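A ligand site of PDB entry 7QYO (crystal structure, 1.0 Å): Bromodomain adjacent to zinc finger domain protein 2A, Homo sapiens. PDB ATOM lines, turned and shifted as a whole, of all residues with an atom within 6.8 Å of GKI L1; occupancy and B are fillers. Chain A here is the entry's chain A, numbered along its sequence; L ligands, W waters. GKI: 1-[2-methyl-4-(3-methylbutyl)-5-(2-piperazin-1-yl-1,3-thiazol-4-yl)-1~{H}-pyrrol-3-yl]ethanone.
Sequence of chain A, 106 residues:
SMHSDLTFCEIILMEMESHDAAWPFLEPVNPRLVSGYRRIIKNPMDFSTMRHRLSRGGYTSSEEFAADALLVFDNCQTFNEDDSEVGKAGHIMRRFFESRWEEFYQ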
ATOM      1  N   TRP A  23      -0.110  12.903   8.867  1.00  0.00           N
ATOM      2  CA  TRP A  23       0.079  11.464   8.705  1.00  0.00           C
ATOM      3  C   TRP A  23      -0.935  10.797   7.774  1.00  0.00           C
ATOM      4  O   TRP A  23      -0.545   9.864   7.065  1.00  0.00           O
ATOM      5  CB  TRP A  23       0.162  10.758  10.076  1.00  0.00           C
ATOM      6  CG  TRP A  23      -1.035  10.945  10.907  1.00  0.00           C
ATOM      7  CD1 TRP A  23      -1.247  11.945  11.813  1.00  0.00           C
ATOM      8  CD2 TRP A  23      -2.232  10.166  10.894  1.00  0.00           C
ATOM      9  NE1 TRP A  23      -2.489  11.848  12.350  1.00  0.00           N
ATOM     10  CE2 TRP A  23      -3.131  10.755  11.812  1.00  0.00           C
ATOM     11  CE3 TRP A  23      -2.646   9.034  10.189  1.00  0.00           C
ATOM     12  CZ2 TRP A  23      -4.391  10.248  12.044  1.00  0.00           C
ATOM     13  CZ3 TRP A  23      -3.908   8.518  10.425  1.00  0.00           C
ATOM     14  CH2 TRP A  23      -4.764   9.140  11.344  1.00  0.00           C
ATOM     15  N   PRO A  24      -2.203  11.230   7.690  1.00  0.00           N
ATOM     16  CA  PRO A  24      -3.108  10.539   6.753  1.00  0.00           C
ATOM     17  C   PRO A  24      -2.771  10.770   5.303  1.00  0.00           C
ATOM     18  O   PRO A  24      -3.237   9.996   4.451  1.00  0.00           O
ATOM     19  CB  PRO A  24      -4.493  11.132   7.063  1.00  0.00           C
ATOM     20  CG  PRO A  24      -4.365  11.721   8.427  1.00  0.00           C
ATOM     21  CD  PRO A  24      -2.943  12.240   8.464  1.00  0.00           C
ATOM     22  N   PHE A  25      -2.034  11.838   4.990  1.00  0.00           N
ATOM     23  CA  PHE A  25      -1.940  12.401   3.646  1.00  0.00           C
ATOM     24  C   PHE A  25      -0.568  12.241   3.022  1.00  0.00           C
ATOM     25  O   PHE A  25      -0.336  12.754   1.917  1.00  0.00           O
ATOM     26  CB  PHE A  25      -2.301  13.911   3.697  1.00  0.00           C
ATOM     27  CG  PHE A  25      -3.565  14.187   4.454  1.00  0.00           C
ATOM     28  CD1 PHE A  25      -4.779  13.745   3.956  1.00  0.00           C
ATOM     29  CD2 PHE A  25      -3.550  14.841   5.683  1.00  0.00           C
ATOM     30  CE1 PHE A  25      -5.950  13.947   4.657  1.00  0.00           C
ATOM     31  CE2 PHE A  25      -4.718  15.036   6.396  1.00  0.00           C
ATOM     32  CZ  PHE A  25      -5.919  14.593   5.877  1.00  0.00           C
ATOM     33  N   LEU A  26       0.343  11.545   3.685  1.00  0.00           N
ATOM     34  CA  LEU A  26       1.724  11.482   3.216  1.00  0.00           C
ATOM     35  C   LEU A  26       1.878  10.677   1.937  1.00  0.00           C
ATOM     36  O   LEU A  26       2.767  10.998   1.127  1.00  0.00           O
ATOM     37  CB  LEU A  26       2.628  10.892   4.298  1.00  0.00           C
ATOM     38  CG  LEU A  26       2.662  11.680   5.616  1.00  0.00           C
ATOM     39  CD1 LEU A  26       3.527  10.969   6.630  1.00  0.00           C
ATOM     40  CD2 LEU A  26       3.127  13.092   5.413  1.00  0.00           C
ATOM     41  N   GLU A  27       1.067   9.641   1.753  1.00  0.00           N
ATOM     42  CA  GLU A  27       1.141   8.723   0.627  1.00  0.00           C
ATOM     43  C   GLU A  27      -0.268   8.516   0.092  1.00  0.00           C
ATOM     44  O   GLU A  27      -1.244   8.821   0.774  1.00  0.00           O
ATOM     45  CB  GLU A  27       1.720   7.377   1.101  1.00  0.00           C
ATOM     46  CG  GLU A  27       3.125   7.474   1.665  1.00  0.00           C
ATOM     47  CD  GLU A  27       4.140   7.763   0.608  1.00  0.00           C
ATOM     48  OE1 GLU A  27       3.894   7.387  -0.557  1.00  0.00           O
ATOM     49  OE2 GLU A  27       5.182   8.369   0.925  1.00  0.00           O
ATOM     50  N   PRO A  28      -0.406   7.980  -1.132  1.00  0.00           N
ATOM     51  CA  PRO A  28      -1.751   7.738  -1.676  1.00  0.00           C
ATOM     52  C   PRO A  28      -2.626   6.967  -0.695  1.00  0.00           C
ATOM     53  O   PRO A  28      -2.160   6.064   0.018  1.00  0.00           O
ATOM     54  CB  PRO A  28      -1.459   6.913  -2.932  1.00  0.00           C
ATOM     55  CG  PRO A  28      -0.099   7.360  -3.362  1.00  0.00           C
ATOM     56  CD  PRO A  28       0.648   7.593  -2.078  1.00  0.00           C
ATOM     57  N   VAL A  29      -3.925   7.276  -0.693  1.00  0.00           N
ATOM     58  CA  VAL A  29      -4.856   6.510   0.129  1.00  0.00           C
ATOM     59  C   VAL A  29      -4.736   5.043  -0.250  1.00  0.00           C
ATOM     60  O   VAL A  29      -4.803   4.687  -1.428  1.00  0.00           O
ATOM     61  CB  VAL A  29      -6.295   7.042   0.000  1.00  0.00           C
ATOM     62  CG1 VAL A  29      -7.263   6.134   0.733  1.00  0.00           C
ATOM     63  CG2 VAL A  29      -6.401   8.455   0.553  1.00  0.00           C
ATOM     64  N   ASN A  30      -4.568   4.193   0.745  1.00  0.00           N
ATOM     65  CA  ASN A  30      -4.069   2.837   0.542  1.00  0.00           C
ATOM     66  C   ASN A  30      -5.221   1.840   0.501  1.00  0.00           C
ATOM     67  O   ASN A  30      -5.892   1.639   1.529  1.00  0.00           O
ATOM     68  CB  ASN A  30      -3.146   2.533   1.727  1.00  0.00           C
ATOM     69  CG  ASN A  30      -2.318   1.272   1.552  1.00  0.00           C
ATOM     70  OD1 ASN A  30      -2.653   0.374   0.765  1.00  0.00           O
ATOM     71  ND2 ASN A  30      -1.235   1.209   2.306  1.00  0.00           N
ATOM     72  N   LEU A  33      -5.829  -0.564   3.342  1.00  0.00           N
ATOM     73  CA  LEU A  33      -6.347  -0.045   4.599  1.00  0.00           C
ATOM     74  C   LEU A  33      -7.780   0.441   4.551  1.00  0.00           C
ATOM     75  O   LEU A  33      -8.410   0.569   5.609  1.00  0.00           O
ATOM     76  CB  LEU A  33      -5.474   1.113   5.105  1.00  0.00           C
ATOM     77  CG  LEU A  33      -3.998   0.778   5.271  1.00  0.00           C
ATOM     78  CD1 LEU A  33      -3.225   1.996   5.743  1.00  0.00           C
ATOM     79  CD2 LEU A  33      -3.774  -0.407   6.235  1.00  0.00           C
ATOM     80  N   VAL A  34      -8.321   0.755   3.368  1.00  0.00           N
ATOM     81  CA  VAL A  34      -9.716   1.227   3.286  1.00  0.00           C
ATOM     82  C   VAL A  34     -10.251   0.840   1.898  1.00  0.00           C
ATOM     83  O   VAL A  34      -9.521   0.988   0.892  1.00  0.00           O
ATOM     84  CB  VAL A  34      -9.780   2.738   3.494  1.00  0.00           C
ATOM     85  CG1 VAL A  34      -8.846   3.471   2.545  1.00  0.00           C
ATOM     86  CG2 VAL A  34     -11.226   3.256   3.459  1.00  0.00           C
ATOM     87  N   SER A  35     -11.488   0.374   1.849  1.00  0.00           N
ATOM     88  CA  SER A  35     -12.134   0.013   0.601  1.00  0.00           C
ATOM     89  C   SER A  35     -13.017   1.159   0.107  1.00  0.00           C
ATOM     90  O   SER A  35     -13.389   2.076   0.843  1.00  0.00           O
ATOM     91  CB  SER A  35     -12.985  -1.249   0.754  1.00  0.00           C
ATOM     92  OG  SER A  35     -14.188  -0.952   1.442  1.00  0.00           O
ATOM     93  N   TYR A  37     -12.576   3.673  -1.869  1.00  0.00           N
ATOM     94  CA  TYR A  37     -12.106   5.059  -1.921  1.00  0.00           C
ATOM     95  C   TYR A  37     -12.165   5.616  -3.334  1.00  0.00           C
ATOM     96  O   TYR A  37     -12.847   6.614  -3.585  1.00  0.00           O
ATOM     97  CB  TYR A  37     -10.696   5.172  -1.316  1.00  0.00           C
ATOM     98  CG  TYR A  37     -10.252   6.619  -1.220  1.00  0.00           C
ATOM     99  CD1 TYR A  37     -10.726   7.431  -0.195  1.00  0.00           C
ATOM    100  CD2 TYR A  37      -9.393   7.168  -2.149  1.00  0.00           C
ATOM    101  CE1 TYR A  37     -10.343   8.754  -0.114  1.00  0.00           C
ATOM    102  CE2 TYR A  37      -9.008   8.500  -2.072  1.00  0.00           C
ATOM    103  CZ  TYR A  37      -9.490   9.286  -1.061  1.00  0.00           C
ATOM    104  OH  TYR A  37      -9.100  10.606  -1.009  1.00  0.00           O
ATOM    105  N   MET A  45      -5.170  12.518  -4.315  1.00  0.00           N
ATOM    106  CA  MET A  45      -3.959  13.307  -4.215  1.00  0.00           C
ATOM    107  C   MET A  45      -3.368  13.114  -2.824  1.00  0.00           C
ATOM    108  O   MET A  45      -4.099  12.891  -1.861  1.00  0.00           O
ATOM    109  CB  MET A  45      -4.231  14.788  -4.508  1.00  0.00           C
ATOM    110  CG  MET A  45      -2.985  15.676  -4.651  1.00  0.00           C
ATOM    111  SD  MET A  45      -1.699  15.045  -5.741  1.00  0.00           S
ATOM    112  CE  MET A  45      -2.590  14.753  -7.258  1.00  0.00           C
ATOM    113  N   VAL A  72      -6.172  17.495  -1.951  1.00  0.00           N
ATOM    114  CA  VAL A  72      -5.989  16.623  -0.790  1.00  0.00           C
ATOM    115  C   VAL A  72      -7.104  16.853   0.222  1.00  0.00           C
ATOM    116  O   VAL A  72      -7.728  15.916   0.734  1.00  0.00           O
ATOM    117  CB  VAL A  72      -4.605  16.831  -0.140  1.00  0.00           C
ATOM    118  CG1 VAL A  72      -4.457  15.964   1.115  1.00  0.00           C
ATOM    119  CG2 VAL A  72      -3.482  16.535  -1.117  1.00  0.00           C
ATOM    120  N   ASN A  75     -10.795  16.146  -1.155  1.00  0.00           N
ATOM    121  CA  ASN A  75     -11.075  14.709  -1.142  1.00  0.00           C
ATOM    122  C   ASN A  75     -11.347  14.216   0.267  1.00  0.00           C
ATOM    123  O   ASN A  75     -12.265  13.421   0.487  1.00  0.00           O
ATOM    124  CB  ASN A  75      -9.895  13.934  -1.726  1.00  0.00           C
ATOM    125  CG  ASN A  75      -9.722  14.138  -3.220  1.00  0.00           C
ATOM    126  OD1 ASN A  75     -10.647  14.562  -3.919  1.00  0.00           O
ATOM    127  ND2 ASN A  75      -8.558  13.766  -3.717  1.00  0.00           N
ATOM    128  N   CYS A  76     -10.560  14.690   1.222  1.00  0.00           N
ATOM    129  CA  CYS A  76     -10.718  14.252   2.603  1.00  0.00           C
ATOM    130  C   CYS A  76     -12.095  14.612   3.135  1.00  0.00           C
ATOM    131  O   CYS A  76     -12.750  13.795   3.798  1.00  0.00           O
ATOM    132  CB  CYS A  76      -9.599  14.864   3.454  1.00  0.00           C
ATOM    133  SG  CYS A  76      -9.610  14.384   5.176  1.00  0.00           S
ATOM    134  N   PHE A  79     -14.875  12.273   1.592  1.00  0.00           N
ATOM    135  CA  PHE A  79     -14.902  10.853   1.922  1.00  0.00           C
ATOM    136  C   PHE A  79     -15.142  10.645   3.413  1.00  0.00           C
ATOM    137  O   PHE A  79     -15.793   9.656   3.785  1.00  0.00           O
ATOM    138  CB  PHE A  79     -13.592  10.139   1.568  1.00  0.00           C
ATOM    139  CG  PHE A  79     -13.719   8.649   1.591  1.00  0.00           C
ATOM    140  CD1 PHE A  79     -14.259   7.998   0.501  1.00  0.00           C
ATOM    141  CD2 PHE A  79     -13.329   7.894   2.697  1.00  0.00           C
ATOM    142  CE1 PHE A  79     -14.401   6.634   0.491  1.00  0.00           C
ATOM    143  CE2 PHE A  79     -13.465   6.517   2.686  1.00  0.00           C
ATOM    144  CZ  PHE A  79     -13.991   5.894   1.569  1.00  0.00           C
ATOM    145  N   ASN A  80     -14.612  11.522   4.259  1.00  0.00           N
ATOM    146  CA  ASN A  80     -14.555  11.277   5.685  1.00  0.00           C
ATOM    147  C   ASN A  80     -15.517  12.174   6.438  1.00  0.00           C
ATOM    148  O   ASN A  80     -15.702  13.333   6.065  1.00  0.00           O
ATOM    149  CB  ASN A  80     -13.143  11.508   6.225  1.00  0.00           C
ATOM    150  CG  ASN A  80     -12.140  10.617   5.566  1.00  0.00           C
ATOM    151  OD1 ASN A  80     -12.054   9.427   5.853  1.00  0.00           O
ATOM    152  ND2 ASN A  80     -11.372  11.190   4.654  1.00  0.00           N
ATOM    153  N   VAL A  86      -9.384  11.220  10.591  1.00  0.00           N
ATOM    154  CA  VAL A  86      -8.819  11.744   9.348  1.00  0.00           C
ATOM    155  C   VAL A  86      -9.558  13.007   8.913  1.00  0.00           C
ATOM    156  O   VAL A  86      -8.936  13.965   8.422  1.00  0.00           O
ATOM    157  CB  VAL A  86      -8.795  10.642   8.262  1.00  0.00           C
ATOM    158  CG1 VAL A  86      -8.391  11.226   6.916  1.00  0.00           C
ATOM    159  CG2 VAL A  86      -7.824   9.528   8.679  1.00  0.00           C
HETATM  160  C11 GKI L   1      -9.034   8.543   3.786  1.00  0.00           C
HETATM  161  C12 GKI L   1     -10.085   7.440   3.570  1.00  0.00           C
HETATM  162  C14 GKI L   1      -6.438  10.328   3.615  1.00  0.00           C
HETATM  163  C15 GKI L   1      -5.302   6.507   6.582  1.00  0.00           C
HETATM  164  C18 GKI L   1      -3.383   5.617   7.309  1.00  0.00           C
HETATM  165  N20 GKI L   1      -1.961   5.314   7.248  1.00  0.00           N
HETATM  166  C25 GKI L   1      -1.099   5.720   6.069  1.00  0.00           C
HETATM  167  C16 GKI L   1      -5.699   5.908   7.817  1.00  0.00           C
HETATM  168  C01 GKI L   1     -10.676   4.361   6.951  1.00  0.00           C
HETATM  169  C02 GKI L   1      -9.750   5.185   7.818  1.00  0.00           C
HETATM  170  C03 GKI L   1      -8.644   4.315   8.503  1.00  0.00           C
HETATM  171  C04 GKI L   1      -9.158   6.370   6.999  1.00  0.00           C
HETATM  172  C05 GKI L   1      -8.387   5.946   5.772  1.00  0.00           C
HETATM  173  C06 GKI L   1      -7.458   7.159   5.273  1.00  0.00           C
HETATM  174  C07 GKI L   1      -6.141   7.349   5.653  1.00  0.00           C
HETATM  175  C09 GKI L   1      -6.629   9.048   4.363  1.00  0.00           C
HETATM  176  C10 GKI L   1      -7.751   8.235   4.478  1.00  0.00           C
HETATM  177  C21 GKI L   1      -1.263   4.659   8.408  1.00  0.00           C
HETATM  178  C22 GKI L   1      -0.025   3.862   8.048  1.00  0.00           C
HETATM  179  C24 GKI L   1       0.183   4.934   5.922  1.00  0.00           C
HETATM  180  N08 GKI L   1      -5.661   8.457   5.098  1.00  0.00           N
HETATM  181  N19 GKI L   1      -3.912   6.389   6.302  1.00  0.00           N
HETATM  182  N23 GKI L   1       0.829   4.576   7.181  1.00  0.00           N
HETATM  183  O13 GKI L   1      -9.211   9.592   3.373  1.00  0.00           O
HETATM  184  S17 GKI L   1      -4.448   5.158   8.512  1.00  0.00           S
HETATM  185  C11 GKI L   2      -2.293   1.786  10.504  1.00  0.00           C
HETATM  186  C12 GKI L   2      -0.988   1.513  11.319  1.00  0.00           C
HETATM  187  C14 GKI L   2      -5.326   1.584   9.622  1.00  0.00           C
HETATM  188  C15 GKI L   2      -5.289   5.060  13.172  1.00  0.00           C
HETATM  189  C18 GKI L   2      -5.544   6.182  15.163  1.00  0.00           C
HETATM  190  N20 GKI L   2      -5.299   6.497  16.576  1.00  0.00           N
HETATM  191  C25 GKI L   2      -4.586   5.535  17.506  1.00  0.00           C
HETATM  192  C16 GKI L   2      -6.302   6.002  12.848  1.00  0.00           C
HETATM  193  C01 GKI L   2       0.282   6.844  11.610  1.00  0.00           C
HETATM  194  C02 GKI L   2      -0.536   6.102  12.644  1.00  0.00           C
HETATM  195  C03 GKI L   2      -1.388   7.078  13.524  1.00  0.00           C
HETATM  196  C04 GKI L   2      -1.450   5.064  11.942  1.00  0.00           C
HETATM  197  C05 GKI L   2      -2.172   4.149  12.905  1.00  0.00           C
HETATM  198  C06 GKI L   2      -3.413   3.562  12.080  1.00  0.00           C
HETATM  199  C07 GKI L   2      -4.735   4.003  12.213  1.00  0.00           C
HETATM  200  C09 GKI L   2      -4.746   2.491  10.650  1.00  0.00           C
HETATM  201  C10 GKI L   2      -3.417   2.607  11.076  1.00  0.00           C
HETATM  202  C21 GKI L   2      -5.679   7.786  17.278  1.00  0.00           C
HETATM  203  C22 GKI L   2      -4.671   8.131  18.375  1.00  0.00           C
HETATM  204  C24 GKI L   2      -4.903   5.778  18.965  1.00  0.00           C
HETATM  205  N08 GKI L   2      -5.511   3.347  11.367  1.00  0.00           N
HETATM  206  N19 GKI L   2      -4.856   5.146  14.552  1.00  0.00           N
HETATM  207  N23 GKI L   2      -4.649   7.151  19.412  1.00  0.00           N
HETATM  208  O13 GKI L   2      -2.413   1.296   9.478  1.00  0.00           O
HETATM  209  S17 GKI L   2      -6.597   6.940  14.128  1.00  0.00           S
HETATM  210  O   HOH W   1      -0.290   8.447   4.265  1.00  0.00           O
HETATM  211  O   HOH W   2       1.244   7.628   7.831  1.00  0.00           O
HETATM  212  O   HOH W   3      -3.571   9.880   1.693  1.00  0.00           O
HETATM  213  O   HOH W   4      -1.546   6.376   2.824  1.00  0.00           O
HETATM  214  O   HOH W   5      -9.176  11.651   1.371  1.00  0.00           O
HETATM  215  O   HOH W   6       2.156   7.366   5.019  1.00  0.00           O
HETATM  216  O   HOH W   7      -4.067   5.321   3.372  1.00  0.00           O
HETATM  217  O   HOH W   8      -0.055   4.025   2.678  1.00  0.00           O
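A sulfur (S17) of GKI L1 sits close to a nitrogen (N08) of GKI L2, 3.5 Å away.
ND2 of Asn 80 sits at hydrogen-bond distance from O of Cys 76, 3.1 Å away. The backbone carbonyl oxygen (O) of Val 86 sits at hydrogen-bond distance from the side-chain sulfur (SG) of Cys 76 (3.3 Å).
Merely in contact with GKI L1: Trp 23 (3.9 Å), Phe 25 (3.8 Å), Val 29 (3.6 Å), Leu 33 (3.9 Å), Val 34 (3.7 Å), Tyr 37 (3.8 Å), Phe 79 (3.4 Å) and Val 86 (3.8 Å). Hydrophobic or aromatic side chains that line GKI L1: Trp 23, Pro 24, Phe 25, Val 29, Leu 33, Val 34, Tyr 37, Phe 79 and Val 86. The nearest printed residue that does not touch GKI L1 is Cys 76 (5.0 Å).
The backbone carbonyl oxygen of Pro 24 sits at hydrogen-bond distance from a nitrogen (N08) of GKI L1. ND2 of Asn 80 is in hydrogen-bond range of O13 of GKI L1.
Water W5 lies within hydrogen-bond range of OH of Tyr 37 (2.6 Å), O13 of GKI L1 (2.9 Å) and N of Cys 76 (3.3 Å). Water W7 lies within hydrogen-bond range of N of Asn 30 and N19 of GKI L1. Water W2 bridges the backbone carbonyl oxygen of Trp 23 (3.0 Å) and a nitrogen (N23) of GKI L1 (3.1 Å).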
